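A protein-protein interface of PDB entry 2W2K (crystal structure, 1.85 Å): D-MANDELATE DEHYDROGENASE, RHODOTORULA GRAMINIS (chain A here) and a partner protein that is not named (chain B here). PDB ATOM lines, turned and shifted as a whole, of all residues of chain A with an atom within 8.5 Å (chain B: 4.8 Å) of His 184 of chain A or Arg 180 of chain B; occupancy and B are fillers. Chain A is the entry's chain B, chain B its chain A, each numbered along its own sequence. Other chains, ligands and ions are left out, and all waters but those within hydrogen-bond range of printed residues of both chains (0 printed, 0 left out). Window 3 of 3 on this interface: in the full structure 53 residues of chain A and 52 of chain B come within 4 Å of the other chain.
The guanidinium group (NH2) of Arg 180 of chain B is in hydrogen-bond range of the backbone carbonyl oxygen (O) of Gly 185 of chain A (3.0 Å). The backbone carbonyl oxygen (O) of His 184 of chain A sits at hydrogen-bond distance from the guanidinium group (NH1) of Arg 180 of chain B. O of Gly 185 of chain B lies within hydrogen-bond range of NH2 of Arg 180 of chain A (3.1 Å). The backbone carbonyl oxygen (O) of His 184 of chain B is in hydrogen-bond range of the guanidinium group (NH1) of Arg 180 of chain A (2.9 Å).
Of the 23 printed residues of chain A, 4 touch a printed residue of chain B. Among the printed residues, 6 pairs touch across the chains.
His 184 of chain A touches just one residue of chain B: Arg 180 (3.0 Å). Of chain A, only His 184 and Gly 185 come within 4 Å of Arg 180 of chain B. No residue of chain A comes within 4 Å of Ala 179 of chain B. Of the printed residues of chain B, Lys 181 of chain A touches Gly 185. Of the printed residues of chain B, Gly 185 of chain A touches Arg 180 and Lys 181. Of the printed residues of chain B, Arg 180 of chain A touches His 184 (2.9 Å) and Gly 185 (3.1 Å). Met 188 of chain A touches none of the printed residues of chain B. Val 183 of chain B touches none of the printed residues of chain A. The nearest printed residue of chain B that does not touch His 184 of chain A is Lys 181 of chain B (6.1 Å). The nearest residue of chain A that does not touch Arg 180 of chain B is Leu 186 of chain A (5.2 Å).
The side-chain carboxylate (OE2) of Glu 177 of chain B is in salt-bridge range of the guanidinium group (NE) of Arg 180 of chain B. The guanidinium group (NE) of Arg 180 of chain A lies within salt-bridge range of the side-chain carboxylate (OE2) of Glu 177 of chain A (3.0 Å). O of Lys 181 of chain A is in hydrogen-bond range of N of Leu 186 of chain A (3.2 Å). NE2 of His 184 of chain A is in hydrogen-bond range of O of Ala 205 of chain A (2.8 Å).
Among the printed residues, merely in contact across the chains: Lys 181 of chain A with Gly 185 of chain B (3.6 Å) and Gly 185 of chain A with Lys 181 of chain B (3.6 Å).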
ATOM      1  N   LEU A 122      26.932  -2.131  17.035  1.00  0.00           N
ATOM      2  CA  LEU A 122      25.626  -2.129  17.731  1.00  0.00           C
ATOM      3  C   LEU A 122      25.368  -3.464  18.461  1.00  0.00           C
ATOM      4  O   LEU A 122      24.860  -3.466  19.597  1.00  0.00           O
ATOM      5  CB  LEU A 122      24.444  -1.791  16.783  1.00  0.00           C
ATOM      6  CG  LEU A 122      23.156  -1.298  17.508  1.00  0.00           C
ATOM      7  CD1 LEU A 122      23.321   0.157  18.007  1.00  0.00           C
ATOM      8  CD2 LEU A 122      21.938  -1.421  16.578  1.00  0.00           C
ATOM      9  N   ARG A 162      18.784   2.475  26.636  1.00  0.00           N
ATOM     10  CA  ARG A 162      17.910   3.665  26.622  1.00  0.00           C
ATOM     11  C   ARG A 162      18.235   4.622  27.779  1.00  0.00           C
ATOM     12  O   ARG A 162      18.268   4.205  28.941  1.00  0.00           O
ATOM     13  CB  ARG A 162      16.414   3.262  26.677  1.00  0.00           C
ATOM     14  CG  ARG A 162      15.442   4.451  26.522  1.00  0.00           C
ATOM     15  CD  ARG A 162      14.001   3.938  26.419  1.00  0.00           C
ATOM     16  NE  ARG A 162      13.026   5.020  26.509  1.00  0.00           N
ATOM     17  N   LYS A 176      29.170   7.863  12.784  1.00  0.00           N
ATOM     18  CA  LYS A 176      27.903   8.554  12.516  1.00  0.00           C
ATOM     19  C   LYS A 176      26.747   7.565  12.364  1.00  0.00           C
ATOM     20  O   LYS A 176      25.620   7.849  12.822  1.00  0.00           O
ATOM     21  CB  LYS A 176      28.004   9.511  11.301  1.00  0.00           C
ATOM     22  CG  LYS A 176      28.896  10.747  11.558  1.00  0.00           C
ATOM     23  CD  LYS A 176      29.001  11.584  10.251  1.00  0.00           C
ATOM     24  CE  LYS A 176      29.824  12.859  10.436  1.00  0.00           C
ATOM     25  NZ  LYS A 176      29.825  13.648   9.147  1.00  0.00           N
ATOM     26  N   GLU A 177      27.032   6.392  11.781  1.00  0.00           N
ATOM     27  CA  GLU A 177      25.999   5.334  11.637  1.00  0.00           C
ATOM     28  C   GLU A 177      25.781   4.563  12.947  1.00  0.00           C
ATOM     29  O   GLU A 177      24.633   4.254  13.285  1.00  0.00           O
ATOM     30  CB  GLU A 177      26.347   4.364  10.491  1.00  0.00           C
ATOM     31  CG  GLU A 177      25.953   4.887   9.087  1.00  0.00           C
ATOM     32  CD  GLU A 177      24.431   4.976   8.912  1.00  0.00           C
ATOM     33  OE1 GLU A 177      23.793   3.916   8.703  1.00  0.00           O
ATOM     34  OE2 GLU A 177      23.874   6.107   8.968  1.00  0.00           O
ATOM     35  N   ILE A 178      26.870   4.227  13.662  1.00  0.00           N
ATOM     36  CA  ILE A 178      26.755   3.718  15.043  1.00  0.00           C
ATOM     37  C   ILE A 178      25.819   4.635  15.888  1.00  0.00           C
ATOM     38  O   ILE A 178      24.846   4.153  16.504  1.00  0.00           O
ATOM     39  CB  ILE A 178      28.156   3.496  15.752  1.00  0.00           C
ATOM     40  CG1 ILE A 178      29.050   2.505  14.961  1.00  0.00           C
ATOM     41  CG2 ILE A 178      27.954   2.995  17.209  1.00  0.00           C
ATOM     42  CD1 ILE A 178      30.507   2.381  15.520  1.00  0.00           C
ATOM     43  N   ALA A 179      26.095   5.951  15.877  1.00  0.00           N
ATOM     44  CA  ALA A 179      25.353   6.929  16.707  1.00  0.00           C
ATOM     45  C   ALA A 179      23.899   7.086  16.266  1.00  0.00           C
ATOM     46  O   ALA A 179      23.005   7.231  17.101  1.00  0.00           O
ATOM     47  CB  ALA A 179      26.071   8.320  16.710  1.00  0.00           C
ATOM     48  N   ARG A 180      23.656   7.074  14.961  1.00  0.00           N
ATOM     49  CA  ARG A 180      22.271   7.178  14.437  1.00  0.00           C
ATOM     50  C   ARG A 180      21.430   5.985  14.959  1.00  0.00           C
ATOM     51  O   ARG A 180      20.288   6.158  15.447  1.00  0.00           O
ATOM     52  CB  ARG A 180      22.261   7.210  12.900  1.00  0.00           C
ATOM     53  CG  ARG A 180      20.850   7.422  12.280  1.00  0.00           C
ATOM     54  CD  ARG A 180      20.834   7.339  10.744  1.00  0.00           C
ATOM     55  NE  ARG A 180      21.211   6.028  10.235  1.00  0.00           N
ATOM     56  CZ  ARG A 180      20.421   4.944  10.242  1.00  0.00           C
ATOM     57  NH1 ARG A 180      19.179   4.993  10.719  1.00  0.00           N
ATOM     58  NH2 ARG A 180      20.880   3.805   9.766  1.00  0.00           N
ATOM     59  N   LYS A 181      22.005   4.791  14.871  1.00  0.00           N
ATOM     60  CA  LYS A 181      21.314   3.568  15.313  1.00  0.00           C
ATOM     61  C   LYS A 181      21.137   3.530  16.855  1.00  0.00           C
ATOM     62  O   LYS A 181      20.055   3.191  17.351  1.00  0.00           O
ATOM     63  CB  LYS A 181      22.034   2.328  14.745  1.00  0.00           C
ATOM     64  CG  LYS A 181      21.933   2.196  13.190  1.00  0.00           C
ATOM     65  CD  LYS A 181      22.950   1.136  12.639  1.00  0.00           C
ATOM     66  CE  LYS A 181      22.953   1.171  11.123  1.00  0.00           C
ATOM     67  NZ  LYS A 181      24.018   0.330  10.493  1.00  0.00           N
ATOM     68  N   ALA A 182      22.175   3.927  17.596  1.00  0.00           N
ATOM     69  CA  ALA A 182      22.121   3.926  19.069  1.00  0.00           C
ATOM     70  C   ALA A 182      21.193   5.007  19.656  1.00  0.00           C
ATOM     71  O   ALA A 182      20.500   4.741  20.650  1.00  0.00           O
ATOM     72  CB  ALA A 182      23.541   4.060  19.670  1.00  0.00           C
ATOM     73  N   VAL A 183      21.192   6.200  19.038  1.00  0.00           N
ATOM     74  CA  VAL A 183      20.373   7.358  19.510  1.00  0.00           C
ATOM     75  C   VAL A 183      18.902   7.243  19.079  1.00  0.00           C
ATOM     76  O   VAL A 183      17.994   7.221  19.928  1.00  0.00           O
ATOM     77  CB  VAL A 183      20.946   8.756  19.029  1.00  0.00           C
ATOM     78  CG1 VAL A 183      19.958   9.898  19.355  1.00  0.00           C
ATOM     79  CG2 VAL A 183      22.321   9.010  19.651  1.00  0.00           C
ATOM     80  N   HIS A 184      18.661   7.169  17.771  1.00  0.00           N
ATOM     81  CA  HIS A 184      17.278   7.083  17.271  1.00  0.00           C
ATOM     82  C   HIS A 184      16.625   5.712  17.477  1.00  0.00           C
ATOM     83  O   HIS A 184      15.436   5.635  17.841  1.00  0.00           O
ATOM     84  CB  HIS A 184      17.200   7.567  15.815  1.00  0.00           C
ATOM     85  CG  HIS A 184      17.617   9.002  15.663  1.00  0.00           C
ATOM     86  ND1 HIS A 184      17.064  10.011  16.425  1.00  0.00           N
ATOM     87  CD2 HIS A 184      18.577   9.585  14.909  1.00  0.00           C
ATOM     88  CE1 HIS A 184      17.645  11.161  16.123  1.00  0.00           C
ATOM     89  NE2 HIS A 184      18.568  10.930  15.207  1.00  0.00           N
ATOM     90  N   GLY A 185      17.401   4.640  17.281  1.00  0.00           N
ATOM     91  CA  GLY A 185      16.903   3.257  17.495  1.00  0.00           C
ATOM     92  C   GLY A 185      16.767   2.869  18.966  1.00  0.00           C
ATOM     93  O   GLY A 185      15.657   2.627  19.433  1.00  0.00           O
ATOM     94  N   LEU A 186      17.885   2.857  19.716  1.00  0.00           N
ATOM     95  CA  LEU A 186      17.884   2.377  21.116  1.00  0.00           C
ATOM     96  C   LEU A 186      17.552   3.434  22.170  1.00  0.00           C
ATOM     97  O   LEU A 186      17.232   3.080  23.312  1.00  0.00           O
ATOM     98  CB  LEU A 186      19.225   1.682  21.499  1.00  0.00           C
ATOM     99  CG  LEU A 186      19.818   0.655  20.510  1.00  0.00           C
ATOM    100  CD1 LEU A 186      21.113   0.043  21.053  1.00  0.00           C
ATOM    101  CD2 LEU A 186      18.790  -0.457  20.196  1.00  0.00           C
ATOM    102  N   GLY A 187      17.609   4.715  21.805  1.00  0.00           N
ATOM    103  CA  GLY A 187      17.261   5.783  22.772  1.00  0.00           C
ATOM    104  C   GLY A 187      18.385   6.314  23.642  1.00  0.00           C
ATOM    105  O   GLY A 187      18.128   6.946  24.694  1.00  0.00           O
ATOM    106  N   MET A 188      19.633   6.085  23.218  1.00  0.00           N
ATOM    107  CA  MET A 188      20.809   6.589  23.955  1.00  0.00           C
ATOM    108  C   MET A 188      20.993   8.103  23.679  1.00  0.00           C
ATOM    109  O   MET A 188      20.350   8.669  22.761  1.00  0.00           O
ATOM    110  CB  MET A 188      22.109   5.813  23.565  1.00  0.00           C
ATOM    111  CG  MET A 188      22.103   4.260  23.821  1.00  0.00           C
ATOM    112  SD  MET A 188      23.738   3.464  23.652  1.00  0.00           S
ATOM    113  CE  MET A 188      24.434   3.958  25.261  1.00  0.00           C
ATOM    114  N   LYS A 189      21.819   8.740  24.516  1.00  0.00           N
ATOM    115  CA  LYS A 189      22.277  10.133  24.364  1.00  0.00           C
ATOM    116  C   LYS A 189      23.753  10.141  23.909  1.00  0.00           C
ATOM    117  O   LYS A 189      24.521   9.256  24.303  1.00  0.00           O
ATOM    118  CB  LYS A 189      22.162  10.881  25.698  1.00  0.00           C
ATOM    119  CG  LYS A 189      20.739  10.914  26.307  1.00  0.00           C
ATOM    120  CD  LYS A 189      20.737  11.496  27.734  1.00  0.00           C
ATOM    121  CE  LYS A 189      19.307  11.592  28.273  1.00  0.00           C
ATOM    122  N   GLU A 201      24.756  19.943  10.806  1.00  0.00           N
ATOM    123  CA  GLU A 201      23.634  19.030  10.560  1.00  0.00           C
ATOM    124  C   GLU A 201      23.771  17.682  11.273  1.00  0.00           C
ATOM    125  O   GLU A 201      22.759  17.114  11.711  1.00  0.00           O
ATOM    126  CB  GLU A 201      23.419  18.831   9.053  1.00  0.00           C
ATOM    127  CG  GLU A 201      22.948  20.102   8.332  1.00  0.00           C
ATOM    128  CD  GLU A 201      21.674  20.685   8.943  1.00  0.00           C
ATOM    129  OE1 GLU A 201      20.692  19.928   9.119  1.00  0.00           O
ATOM    130  OE2 GLU A 201      21.662  21.895   9.255  1.00  0.00           O
ATOM    131  N   THR A 202      24.999  17.160  11.363  1.00  0.00           N
ATOM    132  CA  THR A 202      25.258  15.957  12.173  1.00  0.00           C
ATOM    133  C   THR A 202      24.916  16.254  13.639  1.00  0.00           C
ATOM    134  O   THR A 202      24.221  15.467  14.289  1.00  0.00           O
ATOM    135  CB  THR A 202      26.728  15.426  12.030  1.00  0.00           C
ATOM    136  OG1 THR A 202      26.924  14.864  10.720  1.00  0.00           O
ATOM    137  CG2 THR A 202      27.039  14.350  13.062  1.00  0.00           C
ATOM    138  N   GLU A 203      25.387  17.397  14.147  1.00  0.00           N
ATOM    139  CA  GLU A 203      25.154  17.755  15.550  1.00  0.00           C
ATOM    140  C   GLU A 203      23.671  17.880  15.882  1.00  0.00           C
ATOM    141  O   GLU A 203      23.219  17.329  16.890  1.00  0.00           O
ATOM    142  CB  GLU A 203      25.955  19.004  15.979  1.00  0.00           C
ATOM    143  CG  GLU A 203      27.419  18.675  16.315  1.00  0.00           C
ATOM    144  CD  GLU A 203      28.097  19.702  17.237  1.00  0.00           C
ATOM    145  OE1 GLU A 203      29.288  19.505  17.587  1.00  0.00           O
ATOM    146  OE2 GLU A 203      27.439  20.701  17.616  1.00  0.00           O
ATOM    147  N   LYS A 204      22.905  18.534  15.006  1.00  0.00           N
ATOM    148  CA  LYS A 204      21.468  18.720  15.239  1.00  0.00           C
ATOM    149  C   LYS A 204      20.692  17.391  15.178  1.00  0.00           C
ATOM    150  O   LYS A 204      19.830  17.143  16.010  1.00  0.00           O
ATOM    151  CB  LYS A 204      20.874  19.742  14.253  1.00  0.00           C
ATOM    152  N   ALA A 205      21.024  16.549  14.203  1.00  0.00           N
ATOM    153  CA  ALA A 205      20.354  15.262  14.000  1.00  0.00           C
ATOM    154  C   ALA A 205      20.559  14.279  15.168  1.00  0.00           C
ATOM    155  O   ALA A 205      19.634  13.545  15.536  1.00  0.00           O
ATOM    156  CB  ALA A 205      20.815  14.634  12.695  1.00  0.00           C
ATOM    157  N   LEU A 206      21.759  14.291  15.751  1.00  0.00           N
ATOM    158  CA  LEU A 206      22.133  13.305  16.783  1.00  0.00           C
ATOM    159  C   LEU A 206      22.004  13.833  18.205  1.00  0.00           C
ATOM    160  O   LEU A 206      22.128  13.073  19.162  1.00  0.00           O
ATOM    161  CB  LEU A 206      23.565  12.784  16.541  1.00  0.00           C
ATOM    162  CG  LEU A 206      23.893  12.040  15.227  1.00  0.00           C
ATOM    163  CD1 LEU A 206      25.403  11.716  15.119  1.00  0.00           C
ATOM    164  CD2 LEU A 206      23.058  10.755  15.081  1.00  0.00           C
ATOM    165  N   GLY A 207      21.742  15.132  18.339  1.00  0.00           N
ATOM    166  CA  GLY A 207      21.790  15.799  19.635  1.00  0.00           C
ATOM    167  C   GLY A 207      23.179  15.705  20.257  1.00  0.00           C
ATOM    168  O   GLY A 207      23.303  15.513  21.472  1.00  0.00           O
ATOM    169  N   LYS B 176       5.984  -4.092  17.618  1.00  0.00           N
ATOM    170  CA  LYS B 176       6.033  -2.724  17.051  1.00  0.00           C
ATOM    171  C   LYS B 176       7.366  -2.005  17.328  1.00  0.00           C
ATOM    172  O   LYS B 176       7.877  -1.286  16.451  1.00  0.00           O
ATOM    173  CB  LYS B 176       4.860  -1.858  17.510  1.00  0.00           C
ATOM    174  CG  LYS B 176       3.513  -2.218  16.842  1.00  0.00           C
ATOM    175  CD  LYS B 176       2.387  -1.309  17.374  1.00  0.00           C
ATOM    176  CE  LYS B 176       1.005  -1.830  16.966  1.00  0.00           C
ATOM    177  N   GLU B 177       7.932  -2.208  18.519  1.00  0.00           N
ATOM    178  CA  GLU B 177       9.290  -1.709  18.821  1.00  0.00           C
ATOM    179  C   GLU B 177      10.378  -2.463  18.033  1.00  0.00           C
ATOM    180  O   GLU B 177      11.331  -1.834  17.537  1.00  0.00           O
ATOM    181  CB  GLU B 177       9.570  -1.692  20.340  1.00  0.00           C
ATOM    182  CG  GLU B 177       9.000  -0.449  21.064  1.00  0.00           C
ATOM    183  CD  GLU B 177       9.667   0.883  20.621  1.00  0.00           C
ATOM    184  OE1 GLU B 177      10.785   1.185  21.078  1.00  0.00           O
ATOM    185  OE2 GLU B 177       9.078   1.622  19.810  1.00  0.00           O
ATOM    186  N   ILE B 178      10.271  -3.792  17.938  1.00  0.00           N
ATOM    187  CA  ILE B 178      11.246  -4.589  17.123  1.00  0.00           C
ATOM    188  C   ILE B 178      11.303  -4.053  15.684  1.00  0.00           C
ATOM    189  O   ILE B 178      12.399  -3.797  15.129  1.00  0.00           O
ATOM    190  CB  ILE B 178      10.916  -6.138  17.094  1.00  0.00           C
ATOM    191  CG1 ILE B 178      10.986  -6.764  18.507  1.00  0.00           C
ATOM    192  CG2 ILE B 178      11.878  -6.865  16.127  1.00  0.00           C
ATOM    193  CD1 ILE B 178      10.466  -8.234  18.597  1.00  0.00           C
ATOM    194  N   ALA B 179      10.121  -3.885  15.091  1.00  0.00           N
ATOM    195  CA  ALA B 179       9.975  -3.333  13.733  1.00  0.00           C
ATOM    196  C   ALA B 179      10.506  -1.912  13.565  1.00  0.00           C
ATOM    197  O   ALA B 179      11.200  -1.634  12.588  1.00  0.00           O
ATOM    198  CB  ALA B 179       8.512  -3.416  13.282  1.00  0.00           C
ATOM    199  N   ARG B 180      10.200  -1.008  14.503  1.00  0.00           N
ATOM    200  CA  ARG B 180      10.709   0.380  14.433  1.00  0.00           C
ATOM    201  C   ARG B 180      12.238   0.364  14.370  1.00  0.00           C
ATOM    202  O   ARG B 180      12.841   1.104  13.578  1.00  0.00           O
ATOM    203  CB  ARG B 180      10.216   1.211  15.637  1.00  0.00           C
ATOM    204  CG  ARG B 180      10.635   2.710  15.586  1.00  0.00           C
ATOM    205  CD  ARG B 180      10.247   3.492  16.875  1.00  0.00           C
ATOM    206  NE  ARG B 180      10.933   3.007  18.088  1.00  0.00           N
ATOM    207  CZ  ARG B 180      12.199   3.285  18.410  1.00  0.00           C
ATOM    208  NH1 ARG B 180      12.965   4.037  17.616  1.00  0.00           N
ATOM    209  NH2 ARG B 180      12.711   2.796  19.534  1.00  0.00           N
ATOM    210  N   LYS B 181      12.853  -0.495  15.191  1.00  0.00           N
ATOM    211  CA  LYS B 181      14.329  -0.562  15.292  1.00  0.00           C
ATOM    212  C   LYS B 181      14.921  -1.241  14.058  1.00  0.00           C
ATOM    213  O   LYS B 181      15.935  -0.794  13.515  1.00  0.00           O
ATOM    214  CB  LYS B 181      14.776  -1.220  16.612  1.00  0.00           C
ATOM    215  CG  LYS B 181      14.380  -0.423  17.898  1.00  0.00           C
ATOM    216  CD  LYS B 181      14.522  -1.251  19.196  1.00  0.00           C
ATOM    217  CE  LYS B 181      13.910  -0.476  20.402  1.00  0.00           C
ATOM    218  NZ  LYS B 181      14.003  -1.168  21.700  1.00  0.00           N
ATOM    219  N   ALA B 182      14.273  -2.300  13.590  1.00  0.00           N
ATOM    220  CA  ALA B 182      14.775  -3.015  12.404  1.00  0.00           C
ATOM    221  C   ALA B 182      14.605  -2.243  11.087  1.00  0.00           C
ATOM    222  O   ALA B 182      15.486  -2.333  10.209  1.00  0.00           O
ATOM    223  CB  ALA B 182      14.146  -4.404  12.305  1.00  0.00           C
ATOM    224  N   VAL B 183      13.484  -1.502  10.956  1.00  0.00           N
ATOM    225  CA  VAL B 183      13.159  -0.743   9.732  1.00  0.00           C
ATOM    226  C   VAL B 183      13.932   0.592   9.658  1.00  0.00           C
ATOM    227  O   VAL B 183      14.731   0.795   8.743  1.00  0.00           O
ATOM    228  CB  VAL B 183      11.612  -0.501   9.551  1.00  0.00           C
ATOM    229  CG1 VAL B 183      11.335   0.400   8.335  1.00  0.00           C
ATOM    230  CG2 VAL B 183      10.858  -1.836   9.347  1.00  0.00           C
ATOM    231  N   HIS B 184      13.723   1.480  10.631  1.00  0.00           N
ATOM    232  CA  HIS B 184      14.415   2.766  10.631  1.00  0.00           C
ATOM    233  C   HIS B 184      15.892   2.672  11.049  1.00  0.00           C
ATOM    234  O   HIS B 184      16.741   3.403  10.519  1.00  0.00           O
ATOM    235  CB  HIS B 184      13.637   3.800  11.457  1.00  0.00           C
ATOM    236  CG  HIS B 184      12.230   3.984  10.982  1.00  0.00           C
ATOM    237  ND1 HIS B 184      11.137   3.859  11.814  1.00  0.00           N
ATOM    238  CD2 HIS B 184      11.735   4.208   9.743  1.00  0.00           C
ATOM    239  CE1 HIS B 184      10.032   4.029  11.110  1.00  0.00           C
ATOM    240  NE2 HIS B 184      10.366   4.242   9.852  1.00  0.00           N
ATOM    241  N   GLY B 185      16.202   1.778  11.980  1.00  0.00           N
ATOM    242  CA  GLY B 185      17.605   1.640  12.433  1.00  0.00           C
ATOM    243  C   GLY B 185      18.429   0.844  11.427  1.00  0.00           C
ATOM    244  O   GLY B 185      19.388   1.376  10.852  1.00  0.00           O
ATOM    245  N   LEU B 206       5.716   2.547   9.784  1.00  0.00           N
ATOM    246  CA  LEU B 206       6.634   1.402   9.692  1.00  0.00           C
ATOM    247  C   LEU B 206       6.801   0.866   8.274  1.00  0.00           C
ATOM    248  O   LEU B 206       7.605  -0.043   8.046  1.00  0.00           O
ATOM    249  CB  LEU B 206       6.163   0.250  10.604  1.00  0.00           C
ATOM    250  CG  LEU B 206       6.193   0.495  12.115  1.00  0.00           C
ATOM    251  CD1 LEU B 206       5.530  -0.653  12.871  1.00  0.00           C
ATOM    252  CD2 LEU B 206       7.625   0.725  12.609  1.00  0.00           C
